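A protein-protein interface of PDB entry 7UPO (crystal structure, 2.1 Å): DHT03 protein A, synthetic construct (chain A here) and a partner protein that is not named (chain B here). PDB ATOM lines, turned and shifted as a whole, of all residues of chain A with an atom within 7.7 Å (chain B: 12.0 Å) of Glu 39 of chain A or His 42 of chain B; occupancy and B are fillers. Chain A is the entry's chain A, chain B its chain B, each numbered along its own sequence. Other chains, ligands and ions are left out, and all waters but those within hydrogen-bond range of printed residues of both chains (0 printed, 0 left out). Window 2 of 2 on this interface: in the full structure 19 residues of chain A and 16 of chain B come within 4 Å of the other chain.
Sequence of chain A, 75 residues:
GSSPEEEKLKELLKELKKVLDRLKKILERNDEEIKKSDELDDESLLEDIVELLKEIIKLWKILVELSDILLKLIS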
ATOM      1  N   GLU A  33      24.356  16.124 -29.057  1.00  0.00           N
ATOM      2  CA  GLU A  33      23.366  16.246 -27.991  1.00  0.00           C
ATOM      3  C   GLU A  33      23.101  14.911 -27.307  1.00  0.00           C
ATOM      4  O   GLU A  33      22.863  14.874 -26.095  1.00  0.00           O
ATOM      5  CB  GLU A  33      22.064  16.824 -28.547  1.00  0.00           C
ATOM      6  CG  GLU A  33      22.156  18.277 -28.993  1.00  0.00           C
ATOM      7  CD  GLU A  33      21.959  19.254 -27.849  1.00  0.00           C
ATOM      8  OE1 GLU A  33      21.109  18.983 -26.974  1.00  0.00           O
ATOM      9  OE2 GLU A  33      22.654  20.291 -27.820  1.00  0.00           O
ATOM     10  N   ILE A  34      23.137  13.809 -28.058  1.00  0.00           N
ATOM     11  CA  ILE A  34      22.852  12.505 -27.469  1.00  0.00           C
ATOM     12  C   ILE A  34      24.043  11.993 -26.663  1.00  0.00           C
ATOM     13  O   ILE A  34      23.863  11.262 -25.681  1.00  0.00           O
ATOM     14  CB  ILE A  34      22.431  11.514 -28.570  1.00  0.00           C
ATOM     15  CG1 ILE A  34      21.149  11.995 -29.251  1.00  0.00           C
ATOM     16  CG2 ILE A  34      22.211  10.123 -28.000  1.00  0.00           C
ATOM     17  CD1 ILE A  34      20.696  11.118 -30.396  1.00  0.00           C
ATOM     18  N   LYS A  36      25.584  13.289 -24.446  1.00  0.00           N
ATOM     19  CA  LYS A  36      25.567  13.751 -23.064  1.00  0.00           C
ATOM     20  C   LYS A  36      25.160  12.657 -22.086  1.00  0.00           C
ATOM     21  O   LYS A  36      25.231  12.881 -20.872  1.00  0.00           O
ATOM     22  CB  LYS A  36      24.634  14.957 -22.929  1.00  0.00           C
ATOM     23  CG  LYS A  36      25.068  16.158 -23.757  1.00  0.00           C
ATOM     24  CD  LYS A  36      24.180  17.368 -23.512  1.00  0.00           C
ATOM     25  CE  LYS A  36      24.659  18.571 -24.309  1.00  0.00           C
ATOM     26  NZ  LYS A  36      23.836  19.783 -24.042  1.00  0.00           N
ATOM     27  N   SER A  37      24.728  11.496 -22.586  1.00  0.00           N
ATOM     28  CA  SER A  37      24.471  10.304 -21.781  1.00  0.00           C
ATOM     29  C   SER A  37      23.380  10.518 -20.738  1.00  0.00           C
ATOM     30  O   SER A  37      22.682  11.538 -20.752  1.00  0.00           O
ATOM     31  CB  SER A  37      25.759   9.834 -21.096  1.00  0.00           C
ATOM     32  OG  SER A  37      26.729   9.428 -22.047  1.00  0.00           O
ATOM     33  N   ASP A  38      23.230   9.547 -19.845  1.00  0.00           N
ATOM     34  CA  ASP A  38      22.263   9.573 -18.733  1.00  0.00           C
ATOM     35  C   ASP A  38      20.858   9.679 -19.334  1.00  0.00           C
ATOM     36  O   ASP A  38      20.569   9.029 -20.351  1.00  0.00           O
ATOM     37  CB  ASP A  38      22.637  10.671 -17.759  1.00  0.00           C
ATOM     38  CG  ASP A  38      24.012  10.468 -17.155  1.00  0.00           C
ATOM     39  OD1 ASP A  38      24.405   9.299 -16.953  1.00  0.00           O
ATOM     40  OD2 ASP A  38      24.701  11.473 -16.885  1.00  0.00           O
ATOM     41  N   GLU A  39      19.968  10.472 -18.743  1.00  0.00           N
ATOM     42  CA  GLU A  39      18.591  10.552 -19.206  1.00  0.00           C
ATOM     43  C   GLU A  39      18.469  11.501 -20.390  1.00  0.00           C
ATOM     44  O   GLU A  39      19.136  12.537 -20.449  1.00  0.00           O
ATOM     45  CB  GLU A  39      17.681  11.007 -18.066  1.00  0.00           C
ATOM     46  CG  GLU A  39      18.226  12.184 -17.276  1.00  0.00           C
ATOM     47  CD  GLU A  39      17.543  12.348 -15.933  1.00  0.00           C
ATOM     48  OE1 GLU A  39      16.663  11.523 -15.607  1.00  0.00           O
ATOM     49  OE2 GLU A  39      17.890  13.298 -15.202  1.00  0.00           O
ATOM     50  N   LEU A  40      17.610  11.137 -21.336  1.00  0.00           N
ATOM     51  CA  LEU A  40      17.367  11.926 -22.537  1.00  0.00           C
ATOM     52  C   LEU A  40      15.957  12.495 -22.492  1.00  0.00           C
ATOM     53  O   LEU A  40      15.003  11.780 -22.168  1.00  0.00           O
ATOM     54  CB  LEU A  40      17.550  11.084 -23.804  1.00  0.00           C
ATOM     55  CG  LEU A  40      18.961  10.622 -24.183  1.00  0.00           C
ATOM     56  CD1 LEU A  40      19.390   9.411 -23.371  1.00  0.00           C
ATOM     57  CD2 LEU A  40      19.047  10.324 -25.674  1.00  0.00           C
ATOM     58  N   ASP A  41      15.829  13.779 -22.814  1.00  0.00           N
ATOM     59  CA  ASP A  41      14.519  14.410 -22.854  1.00  0.00           C
ATOM     60  C   ASP A  41      13.748  13.948 -24.083  1.00  0.00           C
ATOM     61  O   ASP A  41      14.307  13.808 -25.176  1.00  0.00           O
ATOM     62  CB  ASP A  41      14.655  15.933 -22.859  1.00  0.00           C
ATOM     63  CG  ASP A  41      13.318  16.639 -22.750  1.00  0.00           C
ATOM     64  OD1 ASP A  41      12.316  15.976 -22.407  1.00  0.00           O
ATOM     65  OD2 ASP A  41      13.264  17.859 -23.010  1.00  0.00           O
ATOM     66  N   ASP A  42      12.448  13.716 -23.897  1.00  0.00           N
ATOM     67  CA  ASP A  42      11.619  13.213 -24.984  1.00  0.00           C
ATOM     68  C   ASP A  42      11.293  14.303 -25.997  1.00  0.00           C
ATOM     69  O   ASP A  42      11.262  14.043 -27.205  1.00  0.00           O
ATOM     70  CB  ASP A  42      10.332  12.616 -24.418  1.00  0.00           C
ATOM     71  CG  ASP A  42      10.595  11.594 -23.333  1.00  0.00           C
ATOM     72  OD1 ASP A  42      11.698  11.009 -23.323  1.00  0.00           O
ATOM     73  OD2 ASP A  42       9.701  11.377 -22.488  1.00  0.00           O
ATOM     74  N   ALA B  35      15.522  -6.602 -26.321  1.00  0.00           N
ATOM     75  CA  ALA B  35      15.360  -5.580 -25.293  1.00  0.00           C
ATOM     76  C   ALA B  35      13.899  -5.198 -25.108  1.00  0.00           C
ATOM     77  O   ALA B  35      13.492  -4.824 -24.003  1.00  0.00           O
ATOM     78  CB  ALA B  35      16.192  -4.347 -25.642  1.00  0.00           C
ATOM     79  N   ALA B  38      12.063  -7.568 -22.726  1.00  0.00           N
ATOM     80  CA  ALA B  38      12.593  -7.576 -21.370  1.00  0.00           C
ATOM     81  C   ALA B  38      12.260  -6.261 -20.680  1.00  0.00           C
ATOM     82  O   ALA B  38      12.246  -5.201 -21.314  1.00  0.00           O
ATOM     83  CB  ALA B  38      14.109  -7.799 -21.369  1.00  0.00           C
ATOM     84  N   GLY B  39      11.988  -6.338 -19.379  1.00  0.00           N
ATOM     85  CA  GLY B  39      11.701  -5.152 -18.595  1.00  0.00           C
ATOM     86  C   GLY B  39      12.927  -4.288 -18.390  1.00  0.00           C
ATOM     87  O   GLY B  39      13.790  -4.607 -17.566  1.00  0.00           O
ATOM     88  N   LEU B  40      13.016  -3.189 -19.132  1.00  0.00           N
ATOM     89  CA  LEU B  40      14.199  -2.344 -19.133  1.00  0.00           C
ATOM     90  C   LEU B  40      13.995  -1.100 -18.277  1.00  0.00           C
ATOM     91  O   LEU B  40      12.897  -0.546 -18.195  1.00  0.00           O
ATOM     92  CB  LEU B  40      14.567  -1.927 -20.557  1.00  0.00           C
ATOM     93  CG  LEU B  40      15.567  -2.813 -21.299  1.00  0.00           C
ATOM     94  CD1 LEU B  40      15.851  -2.243 -22.678  1.00  0.00           C
ATOM     95  CD2 LEU B  40      16.852  -2.947 -20.498  1.00  0.00           C
ATOM     96  N   ASP B  41      15.082  -0.668 -17.643  1.00  0.00           N
ATOM     97  CA  ASP B  41      15.099   0.583 -16.908  1.00  0.00           C
ATOM     98  C   ASP B  41      15.092   1.760 -17.885  1.00  0.00           C
ATOM     99  O   ASP B  41      15.225   1.595 -19.102  1.00  0.00           O
ATOM    100  CB  ASP B  41      16.328   0.639 -16.000  1.00  0.00           C
ATOM    101  CG  ASP B  41      16.213   1.691 -14.916  1.00  0.00           C
ATOM    102  OD1 ASP B  41      15.211   2.437 -14.908  1.00  0.00           O
ATOM    103  OD2 ASP B  41      17.128   1.770 -14.068  1.00  0.00           O
ATOM    104  N   HIS B  42      14.924   2.968 -17.342  1.00  0.00           N
ATOM    105  CA  HIS B  42      15.019   4.155 -18.184  1.00  0.00           C
ATOM    106  C   HIS B  42      16.433   4.337 -18.723  1.00  0.00           C
ATOM    107  O   HIS B  42      16.616   4.902 -19.808  1.00  0.00           O
ATOM    108  CB  HIS B  42      14.577   5.398 -17.412  1.00  0.00           C
ATOM    109  CG  HIS B  42      14.582   6.648 -18.236  1.00  0.00           C
ATOM    110  ND1 HIS B  42      15.298   7.770 -17.881  1.00  0.00           N
ATOM    111  CD2 HIS B  42      13.971   6.946 -19.407  1.00  0.00           C
ATOM    112  CE1 HIS B  42      15.121   8.710 -18.793  1.00  0.00           C
ATOM    113  NE2 HIS B  42      14.320   8.235 -19.731  1.00  0.00           N
ATOM    114  N   GLU B  43      17.440   3.866 -17.982  1.00  0.00           N
ATOM    115  CA  GLU B  43      18.805   3.848 -18.492  1.00  0.00           C
ATOM    116  C   GLU B  43      19.002   2.745 -19.524  1.00  0.00           C
ATOM    117  O   GLU B  43      19.823   2.892 -20.436  1.00  0.00           O
ATOM    118  CB  GLU B  43      19.796   3.671 -17.341  1.00  0.00           C
ATOM    119  CG  GLU B  43      19.574   4.615 -16.174  1.00  0.00           C
ATOM    120  CD  GLU B  43      20.490   4.318 -15.003  1.00  0.00           C
ATOM    121  OE1 GLU B  43      21.612   3.822 -15.236  1.00  0.00           O
ATOM    122  OE2 GLU B  43      20.085   4.575 -13.849  1.00  0.00           O
ATOM    123  N   GLY B  44      18.271   1.636 -19.389  1.00  0.00           N
ATOM    124  CA  GLY B  44      18.334   0.593 -20.398  1.00  0.00           C
ATOM    125  C   GLY B  44      17.730   1.034 -21.717  1.00  0.00           C
ATOM    126  O   GLY B  44      18.255   0.717 -22.787  1.00  0.00           O
ATOM    127  N   ASP B  45      16.619   1.773 -21.658  1.00  0.00           N
ATOM    128  CA  ASP B  45      16.069   2.372 -22.869  1.00  0.00           C
ATOM    129  C   ASP B  45      17.014   3.411 -23.452  1.00  0.00           C
ATOM    130  O   ASP B  45      17.000   3.654 -24.663  1.00  0.00           O
ATOM    131  CB  ASP B  45      14.708   3.004 -22.573  1.00  0.00           C
ATOM    132  CG  ASP B  45      13.687   1.992 -22.095  1.00  0.00           C
ATOM    133  OD1 ASP B  45      13.950   0.777 -22.217  1.00  0.00           O
ATOM    134  OD2 ASP B  45      12.623   2.413 -21.593  1.00  0.00           O
ATOM    135  N   SER B  46      17.844   4.030 -22.608  1.00  0.00           N
ATOM    136  CA  SER B  46      18.783   5.038 -23.089  1.00  0.00           C
ATOM    137  C   SER B  46      19.886   4.406 -23.930  1.00  0.00           C
ATOM    138  O   SER B  46      20.178   4.873 -25.037  1.00  0.00           O
ATOM    139  CB  SER B  46      19.379   5.803 -21.907  1.00  0.00           C
ATOM    140  OG  SER B  46      20.469   6.610 -22.319  1.00  0.00           O
ATOM    141  N   ARG B  47      20.514   3.344 -23.420  1.00  0.00           N
ATOM    142  CA  ARG B  47      21.581   2.696 -24.176  1.00  0.00           C
ATOM    143  C   ARG B  47      21.051   2.055 -25.451  1.00  0.00           C
ATOM    144  O   ARG B  47      21.767   2.001 -26.459  1.00  0.00           O
ATOM    145  CB  ARG B  47      22.297   1.656 -23.310  1.00  0.00           C
ATOM    146  CG  ARG B  47      21.474   0.418 -22.988  1.00  0.00           C
ATOM    147  CD  ARG B  47      22.266  -0.584 -22.161  1.00  0.00           C
ATOM    148  NE  ARG B  47      23.515  -0.974 -22.813  1.00  0.00           N
ATOM    149  CZ  ARG B  47      24.342  -1.904 -22.347  1.00  0.00           C
ATOM    150  NH1 ARG B  47      24.054  -2.550 -21.224  1.00  0.00           N
ATOM    151  NH2 ARG B  47      25.457  -2.193 -23.006  1.00  0.00           N
ATOM    152  N   ILE B  48      19.803   1.581 -25.436  1.00  0.00           N
ATOM    153  CA  ILE B  48      19.215   1.005 -26.639  1.00  0.00           C
ATOM    154  C   ILE B  48      19.027   2.078 -27.702  1.00  0.00           C
ATOM    155  O   ILE B  48      19.368   1.879 -28.873  1.00  0.00           O
ATOM    156  CB  ILE B  48      17.888   0.299 -26.306  1.00  0.00           C
ATOM    157  CG1 ILE B  48      18.157  -0.997 -25.541  1.00  0.00           C
ATOM    158  CG2 ILE B  48      17.096   0.019 -27.574  1.00  0.00           C
ATOM    159  CD1 ILE B  48      19.008  -1.989 -26.308  1.00  0.00           C
ATOM    160  N   PHE B  49      18.497   3.240 -27.307  1.00  0.00           N
ATOM    161  CA  PHE B  49      18.311   4.321 -28.269  1.00  0.00           C
ATOM    162  C   PHE B  49      19.647   4.817 -28.809  1.00  0.00           C
ATOM    163  O   PHE B  49      19.772   5.099 -30.007  1.00  0.00           O
ATOM    164  CB  PHE B  49      17.536   5.479 -27.640  1.00  0.00           C
ATOM    165  CG  PHE B  49      17.408   6.671 -28.546  1.00  0.00           C
ATOM    166  CD1 PHE B  49      16.462   6.686 -29.559  1.00  0.00           C
ATOM    167  CD2 PHE B  49      18.241   7.768 -28.397  1.00  0.00           C
ATOM    168  CE1 PHE B  49      16.344   7.774 -30.402  1.00  0.00           C
ATOM    169  CE2 PHE B  49      18.129   8.860 -29.238  1.00  0.00           C
ATOM    170  CZ  PHE B  49      17.178   8.863 -30.242  1.00  0.00           C
ATOM    171  N   LYS B  50      20.654   4.941 -27.942  1.00  0.00           N
ATOM    172  CA  LYS B  50      21.971   5.374 -28.399  1.00  0.00           C
ATOM    173  C   LYS B  50      22.568   4.368 -29.376  1.00  0.00           C
ATOM    174  O   LYS B  50      23.248   4.749 -30.336  1.00  0.00           O
ATOM    175  CB  LYS B  50      22.898   5.589 -27.202  1.00  0.00           C
ATOM    176  CG  LYS B  50      22.578   6.844 -26.397  1.00  0.00           C
ATOM    177  CD  LYS B  50      23.544   7.045 -25.235  1.00  0.00           C
ATOM    178  CE  LYS B  50      23.277   6.060 -24.108  1.00  0.00           C
ATOM    179  NZ  LYS B  50      24.102   6.355 -22.904  1.00  0.00           N
ATOM    180  N   LYS B  51      22.318   3.078 -29.148  1.00  0.00           N
ATOM    181  CA  LYS B  51      22.761   2.056 -30.089  1.00  0.00           C
ATOM    182  C   LYS B  51      22.055   2.214 -31.431  1.00  0.00           C
ATOM    183  O   LYS B  51      22.687   2.148 -32.491  1.00  0.00           O
ATOM    184  CB  LYS B  51      22.503   0.668 -29.504  1.00  0.00           C
ATOM    185  CG  LYS B  51      23.235  -0.471 -30.193  1.00  0.00           C
ATOM    186  CD  LYS B  51      24.719  -0.455 -29.864  1.00  0.00           C
ATOM    187  CE  LYS B  51      25.347  -1.825 -30.071  1.00  0.00           C
ATOM    188  NZ  LYS B  51      24.822  -2.834 -29.104  1.00  0.00           N
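Of the 9 printed residues of chain A, 4 touch a printed residue of chain B.
Printed residues of chain B that touch a printed residue of chain A: His 42, Ser 46, Phe 49 and Lys 50.
Among the printed residues, 6 pairs touch across the chains.
Among the printed residues, no Asp or Glu carboxylate lies within 4 Å of a Lys or Arg side-chain nitrogen of the other chain.
Among the printed residues, merely in contact across the chains: Leu 40 of chain A with Ser 46 of chain B, Glu 39 of chain A with His 42 of chain B, Ile 34 of chain A with Phe 49 of chain B, Ile 34 of chain A with Lys 50 of chain B and Leu 40 of chain A with Phe 49 of chain B.
OG of Ser 46 of chain B sits at hydrogen-bond distance from O of Asp 38 of chain A (3.1 Å).
Of the printed residues of chain B, Ile 34 of chain A touches Phe 49 (3.6 Å) and Lys 50 (3.7 Å).
No residue of chain B comes within 4 Å of Ser 37 of chain A.
Asp 38 of chain A touches one residue of chain B.
Printed residues of chain B within 4 Å of Glu 39 of chain A: His 42 (3.5 Å).
Leu 40 of chain A touches two residues of chain B.
Of the printed residues of chain A, Ser 46 of chain B touches Asp 38 and Leu 40.
Printed residues of chain A within 4 Å of Phe 49 of chain B: Ile 34 and Leu 40.
Printed residues of chain A within 4 Å of Lys 50 of chain B: Ile 34.
The nearest residue of chain A that does not touch His 42 of chain B is Leu 40 of chain A (4.3 Å).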
